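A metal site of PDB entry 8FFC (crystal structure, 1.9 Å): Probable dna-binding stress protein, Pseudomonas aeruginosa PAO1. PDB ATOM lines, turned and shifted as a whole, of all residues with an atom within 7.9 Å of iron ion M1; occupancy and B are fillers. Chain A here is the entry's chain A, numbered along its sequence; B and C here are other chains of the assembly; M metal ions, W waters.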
ATOM      1  N   ALA A  60      21.813  -2.211 -26.759  1.00  0.00           N
ATOM      2  CA  ALA A  60      22.132  -3.322 -27.663  1.00  0.00           C
ATOM      3  C   ALA A  60      22.163  -4.638 -26.911  1.00  0.00           C
ATOM      4  O   ALA A  60      21.685  -5.671 -27.426  1.00  0.00           O
ATOM      5  CB  ALA A  60      23.462  -3.059 -28.362  1.00  0.00           C
ATOM      6  N   VAL A  61      22.700  -4.657 -25.702  1.00  0.00           N
ATOM      7  CA  VAL A  61      22.634  -5.870 -24.881  1.00  0.00           C
ATOM      8  C   VAL A  61      21.195  -6.188 -24.504  1.00  0.00           C
ATOM      9  O   VAL A  61      20.774  -7.356 -24.524  1.00  0.00           O
ATOM     10  CB  VAL A  61      23.526  -5.728 -23.645  1.00  0.00           C
ATOM     11  CG1 VAL A  61      23.346  -6.964 -22.759  1.00  0.00           C
ATOM     12  CG2 VAL A  61      24.973  -5.543 -24.077  1.00  0.00           C
ATOM     13  N   VAL A  63      18.425  -5.563 -26.143  1.00  0.00           N
ATOM     14  CA  VAL A  63      17.742  -6.150 -27.304  1.00  0.00           C
ATOM     15  C   VAL A  63      18.002  -7.647 -27.365  1.00  0.00           C
ATOM     16  O   VAL A  63      17.094  -8.475 -27.590  1.00  0.00           O
ATOM     17  CB  VAL A  63      18.220  -5.432 -28.591  1.00  0.00           C
ATOM     18  CG1 VAL A  63      17.974  -6.245 -29.841  1.00  0.00           C
ATOM     19  CG2 VAL A  63      17.563  -4.075 -28.712  1.00  0.00           C
ATOM     20  N   ASP A  64      19.260  -8.023 -27.189  1.00  0.00           N
ATOM     21  CA  ASP A  64      19.616  -9.426 -27.285  1.00  0.00           C
ATOM     22  C   ASP A  64      18.949 -10.213 -26.185  1.00  0.00           C
ATOM     23  O   ASP A  64      18.417 -11.309 -26.420  1.00  0.00           O
ATOM     24  CB  ASP A  64      21.134  -9.573 -27.248  1.00  0.00           C
ATOM     25  CG  ASP A  64      21.592 -10.953 -27.641  1.00  0.00           C
ATOM     26  OD1 ASP A  64      21.476 -11.286 -28.847  1.00  0.00           O
ATOM     27  OD2 ASP A  64      22.043 -11.718 -26.743  1.00  0.00           O
ATOM     28  N   ASP A  65      18.931  -9.661 -24.971  1.00  0.00           N
ATOM     29  CA  ASP A  65      18.344 -10.391 -23.853  1.00  0.00           C
ATOM     30  C   ASP A  65      16.835 -10.571 -24.021  1.00  0.00           C
ATOM     31  O   ASP A  65      16.298 -11.644 -23.737  1.00  0.00           O
ATOM     32  CB  ASP A  65      18.637  -9.684 -22.538  1.00  0.00           C
ATOM     33  CG  ASP A  65      20.097  -9.832 -22.080  1.00  0.00           C
ATOM     34  OD1 ASP A  65      20.824 -10.752 -22.554  1.00  0.00           O
ATOM     35  OD2 ASP A  65      20.521  -9.006 -21.246  1.00  0.00           O
ATOM     36  N   ALA A  67      15.123 -10.560 -26.950  1.00  0.00           N
ATOM     37  CA  ALA A  67      14.895 -11.488 -28.060  1.00  0.00           C
ATOM     38  C   ALA A  67      15.155 -12.934 -27.635  1.00  0.00           C
ATOM     39  O   ALA A  67      14.391 -13.844 -28.006  1.00  0.00           O
ATOM     40  CB  ALA A  67      15.786 -11.105 -29.229  1.00  0.00           C
ATOM     41  N   GLU A  68      16.194 -13.159 -26.839  1.00  0.00           N
ATOM     42  CA  GLU A  68      16.488 -14.531 -26.424  1.00  0.00           C
ATOM     43  C   GLU A  68      15.508 -15.025 -25.358  1.00  0.00           C
ATOM     44  O   GLU A  68      15.324 -16.245 -25.227  1.00  0.00           O
ATOM     45  CB  GLU A  68      17.944 -14.636 -25.958  1.00  0.00           C
ATOM     46  CG  GLU A  68      18.880 -14.282 -27.140  1.00  0.00           C
ATOM     47  CD  GLU A  68      20.364 -14.573 -26.946  1.00  0.00           C
ATOM     48  OE1 GLU A  68      20.828 -14.758 -25.814  1.00  0.00           O
ATOM     49  OE2 GLU A  68      21.048 -14.587 -27.978  1.00  0.00           O
ATOM     50  N   HIS B  34      21.815 -10.091 -36.736  1.00  0.00           N
ATOM     51  CA  HIS B  34      21.316 -10.206 -35.376  1.00  0.00           C
ATOM     52  C   HIS B  34      20.078 -11.088 -35.323  1.00  0.00           C
ATOM     53  O   HIS B  34      19.932 -11.934 -34.423  1.00  0.00           O
ATOM     54  CB  HIS B  34      20.987  -8.814 -34.843  1.00  0.00           C
ATOM     55  CG  HIS B  34      21.333  -8.601 -33.400  1.00  0.00           C
ATOM     56  ND1 HIS B  34      21.292  -9.609 -32.467  1.00  0.00           N
ATOM     57  CD2 HIS B  34      21.751  -7.497 -32.750  1.00  0.00           C
ATOM     58  CE1 HIS B  34      21.655  -9.132 -31.289  1.00  0.00           C
ATOM     59  NE2 HIS B  34      21.936  -7.847 -31.434  1.00  0.00           N
ATOM     60  N   HIS B  37      21.175 -14.713 -35.833  1.00  0.00           N
ATOM     61  CA  HIS B  37      21.767 -15.095 -34.539  1.00  0.00           C
ATOM     62  C   HIS B  37      20.716 -15.632 -33.552  1.00  0.00           C
ATOM     63  O   HIS B  37      20.938 -16.671 -32.910  1.00  0.00           O
ATOM     64  CB  HIS B  37      22.498 -13.871 -33.975  1.00  0.00           C
ATOM     65  CG  HIS B  37      22.859 -13.971 -32.524  1.00  0.00           C
ATOM     66  ND1 HIS B  37      23.929 -14.705 -32.070  1.00  0.00           N
ATOM     67  CD2 HIS B  37      22.341 -13.336 -31.442  1.00  0.00           C
ATOM     68  CE1 HIS B  37      24.029 -14.556 -30.755  1.00  0.00           C
ATOM     69  NE2 HIS B  37      23.079 -13.735 -30.351  1.00  0.00           N
ATOM     70  N   TRP B  38      19.594 -14.921 -33.384  1.00  0.00           N
ATOM     71  CA  TRP B  38      18.548 -15.347 -32.452  1.00  0.00           C
ATOM     72  C   TRP B  38      17.796 -16.571 -32.962  1.00  0.00           C
ATOM     73  O   TRP B  38      17.364 -17.412 -32.157  1.00  0.00           O
ATOM     74  CB  TRP B  38      17.517 -14.252 -32.238  1.00  0.00           C
ATOM     75  CG  TRP B  38      18.035 -13.003 -31.686  1.00  0.00           C
ATOM     76  CD1 TRP B  38      19.008 -12.869 -30.722  1.00  0.00           C
ATOM     77  CD2 TRP B  38      17.635 -11.681 -32.045  1.00  0.00           C
ATOM     78  NE1 TRP B  38      19.235 -11.540 -30.467  1.00  0.00           N
ATOM     79  CE2 TRP B  38      18.403 -10.789 -31.266  1.00  0.00           C
ATOM     80  CE3 TRP B  38      16.710 -11.171 -32.954  1.00  0.00           C
ATOM     81  CZ2 TRP B  38      18.270  -9.411 -31.371  1.00  0.00           C
ATOM     82  CZ3 TRP B  38      16.577  -9.793 -33.058  1.00  0.00           C
ATOM     83  CH2 TRP B  38      17.360  -8.929 -32.275  1.00  0.00           C
ATOM     84  N   HIS B  49      25.194 -19.354 -34.133  1.00  0.00           N
ATOM     85  CA  HIS B  49      24.866 -18.370 -33.101  1.00  0.00           C
ATOM     86  C   HIS B  49      26.105 -17.546 -32.740  1.00  0.00           C
ATOM     87  O   HIS B  49      26.048 -16.309 -32.686  1.00  0.00           O
ATOM     88  CB  HIS B  49      24.288 -19.100 -31.898  1.00  0.00           C
ATOM     89  CG  HIS B  49      23.773 -18.228 -30.787  1.00  0.00           C
ATOM     90  ND1 HIS B  49      22.596 -17.513 -30.859  1.00  0.00           N
ATOM     91  CD2 HIS B  49      24.234 -18.065 -29.517  1.00  0.00           C
ATOM     92  CE1 HIS B  49      22.367 -16.926 -29.689  1.00  0.00           C
ATOM     93  NE2 HIS B  49      23.345 -17.249 -28.862  1.00  0.00           N
ATOM     94  N   GLU B  53      27.083 -13.660 -33.997  1.00  0.00           N
ATOM     95  CA  GLU B  53      27.335 -12.667 -32.950  1.00  0.00           C
ATOM     96  C   GLU B  53      28.618 -11.878 -33.206  1.00  0.00           C
ATOM     97  O   GLU B  53      28.649 -10.649 -33.039  1.00  0.00           O
ATOM     98  CB  GLU B  53      27.407 -13.351 -31.587  1.00  0.00           C
ATOM     99  CG  GLU B  53      27.612 -12.404 -30.436  1.00  0.00           C
ATOM    100  CD  GLU B  53      27.645 -13.150 -29.108  1.00  0.00           C
ATOM    101  OE1 GLU B  53      28.625 -13.877 -28.864  1.00  0.00           O
ATOM    102  OE2 GLU B  53      26.676 -13.062 -28.319  1.00  0.00           O
ATOM    103  N   TYR B  56      27.768  -9.399 -36.106  1.00  0.00           N
ATOM    104  CA  TYR B  56      26.961  -8.205 -35.821  1.00  0.00           C
ATOM    105  C   TYR B  56      27.679  -7.297 -34.845  1.00  0.00           C
ATOM    106  O   TYR B  56      27.500  -6.073 -34.893  1.00  0.00           O
ATOM    107  CB  TYR B  56      25.549  -8.571 -35.343  1.00  0.00           C
ATOM    108  CG  TYR B  56      25.327  -8.957 -33.883  1.00  0.00           C
ATOM    109  CD1 TYR B  56      25.633  -8.092 -32.844  1.00  0.00           C
ATOM    110  CD2 TYR B  56      24.775 -10.205 -33.548  1.00  0.00           C
ATOM    111  CE1 TYR B  56      25.428  -8.456 -31.515  1.00  0.00           C
ATOM    112  CE2 TYR B  56      24.564 -10.561 -32.223  1.00  0.00           C
ATOM    113  CZ  TYR B  56      24.910  -9.683 -31.214  1.00  0.00           C
ATOM    114  OH  TYR B  56      24.703  -9.999 -29.894  1.00  0.00           O
ATOM    115  N   LYS C 145      16.835 -20.622 -20.546  1.00  0.00           N
ATOM    116  CA  LYS C 145      17.683 -20.215 -21.661  1.00  0.00           C
ATOM    117  C   LYS C 145      18.536 -21.382 -22.160  1.00  0.00           C
ATOM    118  O   LYS C 145      18.642 -21.617 -23.368  1.00  0.00           O
ATOM    119  CB  LYS C 145      18.535 -19.018 -21.263  1.00  0.00           C
ATOM    120  CG  LYS C 145      19.554 -18.575 -22.326  1.00  0.00           C
ATOM    121  CD  LYS C 145      20.415 -17.403 -21.862  1.00  0.00           C
ATOM    122  CE  LYS C 145      21.412 -17.045 -22.948  1.00  0.00           C
ATOM    123  NZ  LYS C 145      22.287 -15.902 -22.554  1.00  0.00           N
ATOM    124  N   TRP C 148      16.579 -23.827 -24.333  1.00  0.00           N
ATOM    125  CA  TRP C 148      16.428 -23.338 -25.716  1.00  0.00           C
ATOM    126  C   TRP C 148      17.683 -23.595 -26.530  1.00  0.00           C
ATOM    127  O   TRP C 148      17.625 -24.078 -27.666  1.00  0.00           O
ATOM    128  CB  TRP C 148      16.075 -21.830 -25.707  1.00  0.00           C
ATOM    129  CG  TRP C 148      16.573 -21.098 -26.945  1.00  0.00           C
ATOM    130  CD1 TRP C 148      16.222 -21.343 -28.241  1.00  0.00           C
ATOM    131  CD2 TRP C 148      17.524 -20.024 -26.977  1.00  0.00           C
ATOM    132  NE1 TRP C 148      16.910 -20.497 -29.089  1.00  0.00           N
ATOM    133  CE2 TRP C 148      17.704 -19.672 -28.342  1.00  0.00           C
ATOM    134  CE3 TRP C 148      18.245 -19.331 -25.998  1.00  0.00           C
ATOM    135  CZ2 TRP C 148      18.583 -18.652 -28.743  1.00  0.00           C
ATOM    136  CZ3 TRP C 148      19.105 -18.300 -26.403  1.00  0.00           C
ATOM    137  CH2 TRP C 148      19.266 -17.967 -27.750  1.00  0.00           C
ATOM    138  N   MET C 149      18.846 -23.254 -25.973  1.00  0.00           N
ATOM    139  CA  MET C 149      20.094 -23.454 -26.702  1.00  0.00           C
ATOM    140  C   MET C 149      20.305 -24.926 -27.018  1.00  0.00           C
ATOM    141  O   MET C 149      20.660 -25.276 -28.157  1.00  0.00           O
ATOM    142  CB  MET C 149      21.243 -22.873 -25.890  1.00  0.00           C
ATOM    143  CG  MET C 149      21.091 -21.385 -25.796  1.00  0.00           C
ATOM    144  SD  MET C 149      22.441 -20.705 -24.933  1.00  0.00           S
ATOM    145  CE  MET C 149      23.413 -20.473 -26.408  1.00  0.00           C
HETATM  146 FE    FE M   1      22.716 -13.263 -28.193  1.00  0.00          FE
HETATM  147 FE    FE M   2      23.575 -15.426 -27.057  1.00  0.00          FE
HETATM  148  O   HOH W   1      24.684 -12.001 -28.287  1.00  0.00           O
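ND1 of His 37 of chain B lies within hydrogen-bond range of O of His 49 of chain B.
NZ of Lys 145 of chain C is in salt-bridge range of OE1 of Glu 68, at 3.8 Å.
OD1 of Asp 64 lies close to NE1 of Trp 38 of chain B (2.8 Å).
His 49 of chain B touches iron ion M1.
Glu 53 of chain B touches iron ion M1.
Five residues have an atom within 4 Å of iron ion M1: Asp 64, Glu 68, His 37 of chain B, His 49 of chain B and Glu 53 of chain B.
The nearest printed residue that does not touch iron ion M1 is Tyr 56 of chain B (4.2 Å).
Iron ion M1 is bound by OE2 of Glu 68 (2.1 Å), OD2 of Asp 64 (2.2 Å), NE2 of His 37 of chain B (2.2 Å), water W1 (2.3 Å) and OD1 of Asp 64 (2.4 Å).
Iron ion M1 has five donor atoms within binding distance.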
